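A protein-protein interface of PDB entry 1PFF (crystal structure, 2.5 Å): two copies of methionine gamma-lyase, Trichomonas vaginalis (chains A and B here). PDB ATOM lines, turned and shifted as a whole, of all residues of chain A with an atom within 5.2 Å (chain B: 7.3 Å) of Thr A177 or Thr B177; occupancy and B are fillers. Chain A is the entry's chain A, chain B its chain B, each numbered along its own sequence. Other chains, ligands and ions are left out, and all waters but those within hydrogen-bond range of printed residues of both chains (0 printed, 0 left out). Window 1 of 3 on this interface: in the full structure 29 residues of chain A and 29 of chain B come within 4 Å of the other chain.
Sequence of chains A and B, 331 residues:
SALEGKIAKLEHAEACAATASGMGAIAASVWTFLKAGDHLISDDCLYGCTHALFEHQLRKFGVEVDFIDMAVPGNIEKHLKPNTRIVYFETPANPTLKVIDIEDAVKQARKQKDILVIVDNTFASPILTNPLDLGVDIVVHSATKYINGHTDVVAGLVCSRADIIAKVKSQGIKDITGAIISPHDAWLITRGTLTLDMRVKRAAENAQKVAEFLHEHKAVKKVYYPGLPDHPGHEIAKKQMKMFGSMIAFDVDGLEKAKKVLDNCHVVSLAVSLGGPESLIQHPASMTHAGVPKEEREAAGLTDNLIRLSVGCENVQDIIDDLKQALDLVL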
ATOM      1  N   MET A  23      29.791  -5.512   9.340  1.00  0.00           N
ATOM      2  CA  MET A  23      29.348  -4.400   8.490  1.00  0.00           C
ATOM      3  C   MET A  23      29.863  -3.049   9.019  1.00  0.00           C
ATOM      4  O   MET A  23      30.284  -2.186   8.245  1.00  0.00           O
ATOM      5  CB  MET A  23      27.815  -4.396   8.357  1.00  0.00           C
ATOM      6  CG  MET A  23      27.270  -3.346   7.385  1.00  0.00           C
ATOM      7  SD  MET A  23      27.668  -3.689   5.638  1.00  0.00           S
ATOM      8  CE  MET A  23      29.021  -2.638   5.397  1.00  0.00           C
ATOM      9  N   GLY A  24      29.847  -2.886  10.339  1.00  0.00           N
ATOM     10  CA  GLY A  24      30.413  -1.705  10.974  1.00  0.00           C
ATOM     11  C   GLY A  24      31.890  -1.515  10.658  1.00  0.00           C
ATOM     12  O   GLY A  24      32.331  -0.387  10.433  1.00  0.00           O
ATOM     13  N   ALA A  27      32.004  -0.567   6.887  1.00  0.00           N
ATOM     14  CA  ALA A  27      31.456   0.787   6.757  1.00  0.00           C
ATOM     15  C   ALA A  27      32.398   1.860   7.289  1.00  0.00           C
ATOM     16  O   ALA A  27      32.626   2.867   6.611  1.00  0.00           O
ATOM     17  CB  ALA A  27      30.090   0.883   7.445  1.00  0.00           C
ATOM     18  N   ALA A  28      32.950   1.648   8.489  1.00  0.00           N
ATOM     19  CA  ALA A  28      33.845   2.631   9.108  1.00  0.00           C
ATOM     20  C   ALA A  28      35.145   2.771   8.335  1.00  0.00           C
ATOM     21  O   ALA A  28      35.808   3.797   8.429  1.00  0.00           O
ATOM     22  CB  ALA A  28      34.146   2.291  10.570  1.00  0.00           C
ATOM     23  N   TRP A  31      33.458   4.471   4.318  1.00  0.00           N
ATOM     24  CA  TRP A  31      32.908   5.833   4.374  1.00  0.00           C
ATOM     25  C   TRP A  31      33.987   6.842   4.797  1.00  0.00           C
ATOM     26  O   TRP A  31      33.985   7.980   4.342  1.00  0.00           O
ATOM     27  CB  TRP A  31      31.728   5.945   5.344  1.00  0.00           C
ATOM     28  CG  TRP A  31      30.456   5.211   4.982  1.00  0.00           C
ATOM     29  CD1 TRP A  31      29.947   4.103   5.609  1.00  0.00           C
ATOM     30  CD2 TRP A  31      29.497   5.572   3.978  1.00  0.00           C
ATOM     31  NE1 TRP A  31      28.746   3.741   5.042  1.00  0.00           N
ATOM     32  CE2 TRP A  31      28.451   4.619   4.029  1.00  0.00           C
ATOM     33  CE3 TRP A  31      29.423   6.593   3.019  1.00  0.00           C
ATOM     34  CZ2 TRP A  31      27.344   4.662   3.171  1.00  0.00           C
ATOM     35  CZ3 TRP A  31      28.316   6.636   2.161  1.00  0.00           C
ATOM     36  CH2 TRP A  31      27.292   5.672   2.250  1.00  0.00           C
ATOM     37  N   GLN A 171      36.659   9.165  13.076  1.00  0.00           N
ATOM     38  CA  GLN A 171      35.658   9.522  12.070  1.00  0.00           C
ATOM     39  C   GLN A 171      34.691   8.372  11.781  1.00  0.00           C
ATOM     40  O   GLN A 171      33.497   8.491  12.021  1.00  0.00           O
ATOM     41  CB  GLN A 171      36.334  10.015  10.789  1.00  0.00           C
ATOM     42  CG  GLN A 171      37.224  11.232  11.009  1.00  0.00           C
ATOM     43  CD  GLN A 171      37.672  11.853   9.716  1.00  0.00           C
ATOM     44  OE1 GLN A 171      36.887  11.952   8.774  1.00  0.00           O
ATOM     45  NE2 GLN A 171      38.934  12.284   9.660  1.00  0.00           N
ATOM     46  N   GLY A 172      35.222   7.251  11.301  1.00  0.00           N
ATOM     47  CA  GLY A 172      34.410   6.101  10.925  1.00  0.00           C
ATOM     48  C   GLY A 172      33.488   5.597  12.022  1.00  0.00           C
ATOM     49  O   GLY A 172      32.305   5.364  11.778  1.00  0.00           O
ATOM     50  N   ILE A 173      34.026   5.426  13.226  1.00  0.00           N
ATOM     51  CA  ILE A 173      33.220   4.944  14.347  1.00  0.00           C
ATOM     52  C   ILE A 173      32.491   6.089  15.051  1.00  0.00           C
ATOM     53  O   ILE A 173      31.269   6.057  15.173  1.00  0.00           O
ATOM     54  CB  ILE A 173      34.073   4.105  15.338  1.00  0.00           C
ATOM     55  CG1 ILE A 173      34.550   2.819  14.663  1.00  0.00           C
ATOM     56  CG2 ILE A 173      33.274   3.775  16.599  1.00  0.00           C
ATOM     57  CD1 ILE A 173      35.745   2.155  15.358  1.00  0.00           C
ATOM     58  N   ASP A 175      31.958   9.412  14.330  1.00  0.00           N
ATOM     59  CA  ASP A 175      31.093  10.323  13.582  1.00  0.00           C
ATOM     60  C   ASP A 175      30.157   9.614  12.604  1.00  0.00           C
ATOM     61  O   ASP A 175      28.949   9.882  12.597  1.00  0.00           O
ATOM     62  CB  ASP A 175      31.906  11.376  12.816  1.00  0.00           C
ATOM     63  CG  ASP A 175      32.716  12.291  13.723  1.00  0.00           C
ATOM     64  OD1 ASP A 175      32.500  12.315  14.953  1.00  0.00           O
ATOM     65  OD2 ASP A 175      33.620  13.023  13.269  1.00  0.00           O
ATOM     66  N   ILE A 176      30.696   8.720  11.779  1.00  0.00           N
ATOM     67  CA  ILE A 176      29.952   8.248  10.611  1.00  0.00           C
ATOM     68  C   ILE A 176      28.941   7.140  10.914  1.00  0.00           C
ATOM     69  O   ILE A 176      27.763   7.259  10.563  1.00  0.00           O
ATOM     70  CB  ILE A 176      30.910   7.832   9.462  1.00  0.00           C
ATOM     71  CG1 ILE A 176      31.680   9.053   8.936  1.00  0.00           C
ATOM     72  CG2 ILE A 176      30.128   7.188   8.322  1.00  0.00           C
ATOM     73  CD1 ILE A 176      33.006   8.704   8.235  1.00  0.00           C
ATOM     74  N   THR A 177      29.404   6.078  11.563  1.00  0.00           N
ATOM     75  CA  THR A 177      28.579   4.881  11.772  1.00  0.00           C
ATOM     76  C   THR A 177      28.014   4.774  13.183  1.00  0.00           C
ATOM     77  O   THR A 177      26.952   4.180  13.378  1.00  0.00           O
ATOM     78  CB  THR A 177      29.390   3.607  11.498  1.00  0.00           C
ATOM     79  OG1 THR A 177      30.478   3.535  12.423  1.00  0.00           O
ATOM     80  CG2 THR A 177      30.055   3.644  10.113  1.00  0.00           C
ATOM     81  N   GLY A 178      28.747   5.294  14.166  1.00  0.00           N
ATOM     82  CA  GLY A 178      28.446   5.023  15.560  1.00  0.00           C
ATOM     83  C   GLY A 178      28.510   3.534  15.897  1.00  0.00           C
ATOM     84  O   GLY A 178      27.903   3.104  16.865  1.00  0.00           O
ATOM     85  N   ALA A 179      29.233   2.748  15.095  1.00  0.00           N
ATOM     86  CA  ALA A 179      29.299   1.287  15.289  1.00  0.00           C
ATOM     87  C   ALA A 179      30.334   0.887  16.343  1.00  0.00           C
ATOM     88  O   ALA A 179      31.335   0.219  16.040  1.00  0.00           O
ATOM     89  CB  ALA A 179      29.552   0.567  13.956  1.00  0.00           C
ATOM     90  N   THR B  19      20.186   0.350  18.407  1.00  0.00           N
ATOM     91  CA  THR B  19      21.486   0.449  17.751  1.00  0.00           C
ATOM     92  C   THR B  19      22.610   0.386  18.770  1.00  0.00           C
ATOM     93  O   THR B  19      22.370   0.409  19.979  1.00  0.00           O
ATOM     94  CB  THR B  19      21.632   1.775  17.007  1.00  0.00           C
ATOM     95  OG1 THR B  19      21.609   2.842  17.963  1.00  0.00           O
ATOM     96  CG2 THR B  19      20.430   2.045  16.089  1.00  0.00           C
ATOM     97  N   ALA B  20      23.837   0.370  18.246  1.00  0.00           N
ATOM     98  CA  ALA B  20      25.058   0.227  19.029  1.00  0.00           C
ATOM     99  C   ALA B  20      25.412   1.449  19.875  1.00  0.00           C
ATOM    100  O   ALA B  20      26.176   1.333  20.833  1.00  0.00           O
ATOM    101  CB  ALA B  20      26.225  -0.117  18.097  1.00  0.00           C
ATOM    102  N   SER B  21      24.868   2.612  19.522  1.00  0.00           N
ATOM    103  CA  SER B  21      25.188   3.863  20.206  1.00  0.00           C
ATOM    104  C   SER B  21      24.258   4.995  19.785  1.00  0.00           C
ATOM    105  O   SER B  21      23.558   4.895  18.774  1.00  0.00           O
ATOM    106  CB  SER B  21      26.636   4.282  19.917  1.00  0.00           C
ATOM    107  OG  SER B  21      26.757   4.763  18.585  1.00  0.00           O
ATOM    108  N   GLY B  22      24.266   6.081  20.557  1.00  0.00           N
ATOM    109  CA  GLY B  22      23.487   7.260  20.212  1.00  0.00           C
ATOM    110  C   GLY B  22      23.863   7.794  18.841  1.00  0.00           C
ATOM    111  O   GLY B  22      22.994   8.161  18.054  1.00  0.00           O
ATOM    112  N   MET B  23      25.160   7.832  18.550  1.00  0.00           N
ATOM    113  CA  MET B  23      25.626   8.251  17.231  1.00  0.00           C
ATOM    114  C   MET B  23      25.089   7.308  16.139  1.00  0.00           C
ATOM    115  O   MET B  23      24.716   7.762  15.056  1.00  0.00           O
ATOM    116  CB  MET B  23      27.161   8.326  17.202  1.00  0.00           C
ATOM    117  CG  MET B  23      27.717   9.584  17.859  1.00  0.00           C
ATOM    118  SD  MET B  23      26.846  11.127  17.381  1.00  0.00           S
ATOM    119  CE  MET B  23      27.224  11.138  15.580  1.00  0.00           C
ATOM    120  N   GLY B  24      25.041   6.005  16.447  1.00  0.00           N
ATOM    121  CA  GLY B  24      24.432   4.998  15.585  1.00  0.00           C
ATOM    122  C   GLY B  24      22.968   5.278  15.244  1.00  0.00           C
ATOM    123  O   GLY B  24      22.540   5.112  14.091  1.00  0.00           O
ATOM    124  N   ALA B  25      22.201   5.696  16.245  1.00  0.00           N
ATOM    125  CA  ALA B  25      20.802   6.065  16.041  1.00  0.00           C
ATOM    126  C   ALA B  25      20.666   7.252  15.086  1.00  0.00           C
ATOM    127  O   ALA B  25      19.861   7.220  14.134  1.00  0.00           O
ATOM    128  CB  ALA B  25      20.152   6.373  17.360  1.00  0.00           C
ATOM    129  N   ILE B  26      21.461   8.283  15.346  1.00  0.00           N
ATOM    130  CA  ILE B  26      21.444   9.499  14.535  1.00  0.00           C
ATOM    131  C   ILE B  26      21.875   9.158  13.110  1.00  0.00           C
ATOM    132  O   ILE B  26      21.200   9.503  12.144  1.00  0.00           O
ATOM    133  CB  ILE B  26      22.362  10.582  15.144  1.00  0.00           C
ATOM    134  CG1 ILE B  26      21.840  10.998  16.528  1.00  0.00           C
ATOM    135  CG2 ILE B  26      22.452  11.799  14.202  1.00  0.00           C
ATOM    136  CD1 ILE B  26      22.881  11.667  17.442  1.00  0.00           C
ATOM    137  N   ALA B  27      22.999   8.461  12.995  1.00  0.00           N
ATOM    138  CA  ALA B  27      23.541   8.098  11.691  1.00  0.00           C
ATOM    139  C   ALA B  27      22.616   7.190  10.889  1.00  0.00           C
ATOM    140  O   ALA B  27      22.380   7.446   9.703  1.00  0.00           O
ATOM    141  CB  ALA B  27      24.939   7.468  11.844  1.00  0.00           C
ATOM    142  N   ALA B  28      22.070   6.148  11.522  1.00  0.00           N
ATOM    143  CA  ALA B  28      21.153   5.248  10.817  1.00  0.00           C
ATOM    144  C   ALA B  28      19.883   5.956  10.334  1.00  0.00           C
ATOM    145  O   ALA B  28      19.276   5.523   9.354  1.00  0.00           O
ATOM    146  CB  ALA B  28      20.788   4.044  11.670  1.00  0.00           C
ATOM    147  N   SER B  29      19.474   7.021  11.026  1.00  0.00           N
ATOM    148  CA  SER B  29      18.348   7.824  10.563  1.00  0.00           C
ATOM    149  C   SER B  29      18.768   8.708   9.375  1.00  0.00           C
ATOM    150  O   SER B  29      18.190   8.608   8.274  1.00  0.00           O
ATOM    151  CB  SER B  29      17.757   8.667  11.704  1.00  0.00           C
ATOM    152  OG  SER B  29      17.461   7.870  12.844  1.00  0.00           O
ATOM    153  N   TRP B  31      21.572   9.039   7.295  1.00  0.00           N
ATOM    154  CA  TRP B  31      22.125   8.446   6.067  1.00  0.00           C
ATOM    155  C   TRP B  31      21.042   7.709   5.258  1.00  0.00           C
ATOM    156  O   TRP B  31      21.109   7.642   4.024  1.00  0.00           O
ATOM    157  CB  TRP B  31      23.264   7.467   6.365  1.00  0.00           C
ATOM    158  CG  TRP B  31      24.563   8.041   6.928  1.00  0.00           C
ATOM    159  CD1 TRP B  31      25.116   7.750   8.146  1.00  0.00           C
ATOM    160  CD2 TRP B  31      25.485   8.944   6.285  1.00  0.00           C
ATOM    161  NE1 TRP B  31      26.306   8.422   8.312  1.00  0.00           N
ATOM    162  CE2 TRP B  31      26.558   9.168   7.191  1.00  0.00           C
ATOM    163  CE3 TRP B  31      25.518   9.590   5.037  1.00  0.00           C
ATOM    164  CZ2 TRP B  31      27.641  10.005   6.892  1.00  0.00           C
ATOM    165  CZ3 TRP B  31      26.600  10.429   4.738  1.00  0.00           C
ATOM    166  CH2 TRP B  31      27.647  10.629   5.672  1.00  0.00           C
ATOM    167  N   THR B  32      20.055   7.150   5.955  1.00  0.00           N
ATOM    168  CA  THR B  32      18.997   6.377   5.295  1.00  0.00           C
ATOM    169  C   THR B  32      18.135   7.252   4.400  1.00  0.00           C
ATOM    170  O   THR B  32      17.715   6.827   3.330  1.00  0.00           O
ATOM    171  CB  THR B  32      18.107   5.672   6.338  1.00  0.00           C
ATOM    172  OG1 THR B  32      18.876   4.669   7.004  1.00  0.00           O
ATOM    173  CG2 THR B  32      16.985   4.871   5.661  1.00  0.00           C
ATOM    174  N   LEU B  53      29.499  14.940  12.336  1.00  0.00           N
ATOM    175  CA  LEU B  53      28.752  14.151  11.353  1.00  0.00           C
ATOM    176  C   LEU B  53      28.129  15.067  10.294  1.00  0.00           C
ATOM    177  O   LEU B  53      28.287  14.832   9.099  1.00  0.00           O
ATOM    178  CB  LEU B  53      27.670  13.293  12.035  1.00  0.00           C
ATOM    179  CG  LEU B  53      26.604  12.675  11.129  1.00  0.00           C
ATOM    180  CD1 LEU B  53      27.168  11.612  10.162  1.00  0.00           C
ATOM    181  CD2 LEU B  53      25.489  12.085  11.954  1.00  0.00           C
ATOM    182  N   VAL B 168      15.117   2.206   8.370  1.00  0.00           N
ATOM    183  CA  VAL B 168      16.218   2.429   9.303  1.00  0.00           C
ATOM    184  C   VAL B 168      16.938   1.116   9.632  1.00  0.00           C
ATOM    185  O   VAL B 168      18.167   1.086   9.724  1.00  0.00           O
ATOM    186  CB  VAL B 168      15.732   3.133  10.604  1.00  0.00           C
ATOM    187  CG1 VAL B 168      16.802   3.093  11.684  1.00  0.00           C
ATOM    188  CG2 VAL B 168      15.334   4.593  10.316  1.00  0.00           C
ATOM    189  N   GLN B 171      18.280  -0.675   5.977  1.00  0.00           N
ATOM    190  CA  GLN B 171      19.283   0.151   5.313  1.00  0.00           C
ATOM    191  C   GLN B 171      20.245   0.804   6.300  1.00  0.00           C
ATOM    192  O   GLN B 171      21.448   0.534   6.269  1.00  0.00           O
ATOM    193  CB  GLN B 171      18.618   1.209   4.427  1.00  0.00           C
ATOM    194  CG  GLN B 171      17.904   0.621   3.212  1.00  0.00           C
ATOM    195  CD  GLN B 171      17.276   1.693   2.353  1.00  0.00           C
ATOM    196  OE1 GLN B 171      17.965   2.592   1.865  1.00  0.00           O
ATOM    197  NE2 GLN B 171      15.967   1.612   2.171  1.00  0.00           N
ATOM    198  N   GLY B 172      19.711   1.640   7.190  1.00  0.00           N
ATOM    199  CA  GLY B 172      20.538   2.407   8.107  1.00  0.00           C
ATOM    200  C   GLY B 172      21.454   1.551   8.958  1.00  0.00           C
ATOM    201  O   GLY B 172      22.641   1.847   9.100  1.00  0.00           O
ATOM    202  N   ILE B 173      20.894   0.493   9.536  1.00  0.00           N
ATOM    203  CA  ILE B 173      21.667  -0.404  10.393  1.00  0.00           C
ATOM    204  C   ILE B 173      22.383  -1.480   9.581  1.00  0.00           C
ATOM    205  O   ILE B 173      23.608  -1.602   9.646  1.00  0.00           O
ATOM    206  CB  ILE B 173      20.779  -1.002  11.524  1.00  0.00           C
ATOM    207  CG1 ILE B 173      20.231   0.124  12.405  1.00  0.00           C
ATOM    208  CG2 ILE B 173      21.574  -2.004  12.376  1.00  0.00           C
ATOM    209  CD1 ILE B 173      19.055  -0.290  13.319  1.00  0.00           C
ATOM    210  N   LYS B 174      21.637  -2.248   8.796  1.00  0.00           N
ATOM    211  CA  LYS B 174      22.219  -3.423   8.146  1.00  0.00           C
ATOM    212  C   LYS B 174      23.169  -3.116   6.986  1.00  0.00           C
ATOM    213  O   LYS B 174      24.116  -3.867   6.763  1.00  0.00           O
ATOM    214  CB  LYS B 174      21.131  -4.411   7.708  1.00  0.00           C
ATOM    215  CG  LYS B 174      20.422  -5.092   8.878  1.00  0.00           C
ATOM    216  CD  LYS B 174      19.423  -6.141   8.396  1.00  0.00           C
ATOM    217  CE  LYS B 174      18.425  -6.506   9.495  1.00  0.00           C
ATOM    218  NZ  LYS B 174      17.754  -7.819   9.225  1.00  0.00           N
ATOM    219  N   ASP B 175      22.926  -2.027   6.260  1.00  0.00           N
ATOM    220  CA  ASP B 175      23.745  -1.691   5.093  1.00  0.00           C
ATOM    221  C   ASP B 175      24.761  -0.588   5.406  1.00  0.00           C
ATOM    222  O   ASP B 175      25.973  -0.764   5.209  1.00  0.00           O
ATOM    223  CB  ASP B 175      22.869  -1.250   3.908  1.00  0.00           C
ATOM    224  CG  ASP B 175      21.991  -2.369   3.350  1.00  0.00           C
ATOM    225  OD1 ASP B 175      22.233  -3.563   3.628  1.00  0.00           O
ATOM    226  OD2 ASP B 175      21.020  -2.126   2.595  1.00  0.00           O
ATOM    227  N   ILE B 176      24.268   0.538   5.907  1.00  0.00           N
ATOM    228  CA  ILE B 176      25.058   1.765   6.002  1.00  0.00           C
ATOM    229  C   ILE B 176      26.020   1.821   7.199  1.00  0.00           C
ATOM    230  O   ILE B 176      27.215   2.047   7.012  1.00  0.00           O
ATOM    231  CB  ILE B 176      24.127   2.999   5.993  1.00  0.00           C
ATOM    232  CG1 ILE B 176      23.284   3.013   4.711  1.00  0.00           C
ATOM    233  CG2 ILE B 176      24.939   4.271   6.108  1.00  0.00           C
ATOM    234  CD1 ILE B 176      22.069   3.937   4.760  1.00  0.00           C
ATOM    235  N   THR B 177      25.503   1.652   8.415  1.00  0.00           N
ATOM    236  CA  THR B 177      26.313   1.854   9.618  1.00  0.00           C
ATOM    237  C   THR B 177      26.877   0.572  10.217  1.00  0.00           C
ATOM    238  O   THR B 177      27.947   0.596  10.804  1.00  0.00           O
ATOM    239  CB  THR B 177      25.545   2.606  10.745  1.00  0.00           C
ATOM    240  OG1 THR B 177      24.381   1.860  11.121  1.00  0.00           O
ATOM    241  CG2 THR B 177      25.007   3.975  10.287  1.00  0.00           C
ATOM    242  N   GLY B 178      26.137  -0.530  10.114  1.00  0.00           N
ATOM    243  CA  GLY B 178      26.464  -1.718  10.890  1.00  0.00           C
ATOM    244  C   GLY B 178      26.402  -1.483  12.400  1.00  0.00           C
ATOM    245  O   GLY B 178      27.022  -2.227  13.156  1.00  0.00           O
ATOM    246  N   ALA B 179      25.658  -0.465  12.841  1.00  0.00           N
ATOM    247  CA  ALA B 179      25.596  -0.114  14.274  1.00  0.00           C
ATOM    248  C   ALA B 179      24.547  -0.953  14.998  1.00  0.00           C
ATOM    249  O   ALA B 179      23.558  -0.442  15.528  1.00  0.00           O
ATOM    250  CB  ALA B 179      25.374   1.382  14.474  1.00  0.00           C
ATOM    251  N   ILE B 180      24.798  -2.260  15.001  1.00  0.00           N
ATOM    252  CA  ILE B 180      23.884  -3.271  15.533  1.00  0.00           C
ATOM    253  C   ILE B 180      24.075  -3.325  17.045  1.00  0.00           C
ATOM    254  O   ILE B 180      25.212  -3.375  17.508  1.00  0.00           O
ATOM    255  CB  ILE B 180      24.216  -4.637  14.864  1.00  0.00           C
ATOM    256  CG1 ILE B 180      23.892  -4.577  13.358  1.00  0.00           C
ATOM    257  CG2 ILE B 180      23.481  -5.803  15.552  1.00  0.00           C
ATOM    258  CD1 ILE B 180      24.461  -5.731  12.522  1.00  0.00           C
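The indole nitrogen (NE1) of Trp A31 is in hydrogen-bond range of the backbone carbonyl oxygen (O) of Ile B176, at 3.0 Å.
NE1 of Trp B31 sits at hydrogen-bond distance from O of Ile A176 (2.9 Å).
The backbone carbonyl oxygen (O) of Gly A178 is in hydrogen-bond range of the side-chain hydroxyl (OG) of Ser B21, 2.7 Å away.
The side-chain sulfur (SD) of Met A23 lies close to the backbone carbonyl oxygen (O) of Lys B174 (3.7 Å).
The side-chain sulfur of Met A23 sits close to the backbone carbonyl oxygen of Asp B175.
N of Ile A176 lies within hydrogen-bond range of O of Gln A171 (2.8 Å).
The side-chain hydroxyl (OG1) of Thr A177 sits close to the backbone NH (N) of Ala A179, 3.1 Å away.
OG1 of Thr B19 lies within hydrogen-bond range of O of Ser B21 (2.9 Å).
The backbone NH (N) of Met B23 lies close to the side-chain hydroxyl (OG) of Ser B21 (3.5 Å).
The backbone NH (N) of Gly B24 is in hydrogen-bond range of the side-chain hydroxyl (OG) of Ser B21, 3.0 Å away.
The backbone carbonyl oxygen (O) of Gln B171 lies within hydrogen-bond range of the backbone NH (N) of Ile B176.
Among the printed residues, pairs that only touch across the chains: Met A23 with Gly B178 (3.9 Å), Gly A24 with Thr B177 (3.4 Å), Gly A24 with Gly B178 (3.6 Å), Ala A27 with Ile B176 (3.1 Å), Ala A27 with Thr B177 (3.99 Å), Asp A175 with Met B23 (3.7 Å), Asp A175 with Leu B53 (3.5 Å), Ile A176 with Ala B27 (3.1 Å), Thr A177 with Gly B24 (3.4 Å), Thr A177 with Thr B177 (3.4 Å), Thr A177 with Ala B179 (3.4 Å), Gly A178 with Ala B20 (3.8 Å), Gly A178 with Met B23 (3.9 Å), Gly A178 with Gly B24 (3.7 Å), Gly A178 with Ala B179 (3.9 Å), Ala A179 with Thr B177 (3.5 Å) and Ala A179 with Gly B178 (3.9 Å).
Of chain B, only Gly B24 (3.4 Å), Thr B177 (3.4 Å) and Ala B179 (3.4 Å) come within 4 Å of Thr A177.
Of the printed residues of chain B, Ala A179 touches Thr B177 and Gly B178.
Printed residues of chain A within 4 Å of Gly B24: Thr A177 (3.4 Å) and Gly A178 (3.7 Å).
Of the printed residues of chain A, Leu B53 touches Asp A175.
Of the printed residues of chain A, Thr B177 touches Gly A24, Ala A27, Thr A177 and Ala A179.
The nearest residue of chain B that does not touch Thr A177 is Ala B27 (4.1 Å).
The nearest printed residue of chain A that does not touch Thr B177 is Ile A176 (4.3 Å).
Of the 25 printed residues of chain B, 13 touch a printed residue of chain A.
Hydrophobic or aromatic side chains of chain B within 4 Å of the printed part of chain A: Ala B20, Met B23, Ala B27, Trp B31, Leu B53, Ile B176 and Ala B179.
Hydrophobic or aromatic side chains of chain A that line the printed part of chain B: Met A23, Ala A27, Trp A31 and Ala A179.
Met A23 touches Asp B175, and with the chains exchanged Asp A175 touches Met B23.
Met A23 touches Gly B178, and with the chains exchanged Gly A178 touches Met B23.
Ala A27 touches Ile B176, and with the chains exchanged Ile A176 touches Ala B27.
Ala A27 touches Thr B177, but with the chains exchanged Thr A177 does not touch Ala B27 (4.1 Å).
Positions printed for both chains: 23, 24, 27, 28, 31, 171, 172, 173, 175, 176, 177, 178 and 179.
Of the 22 pairs that touch across the chains among the printed residues, 17 have their exchanged pair printed and touching as well.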
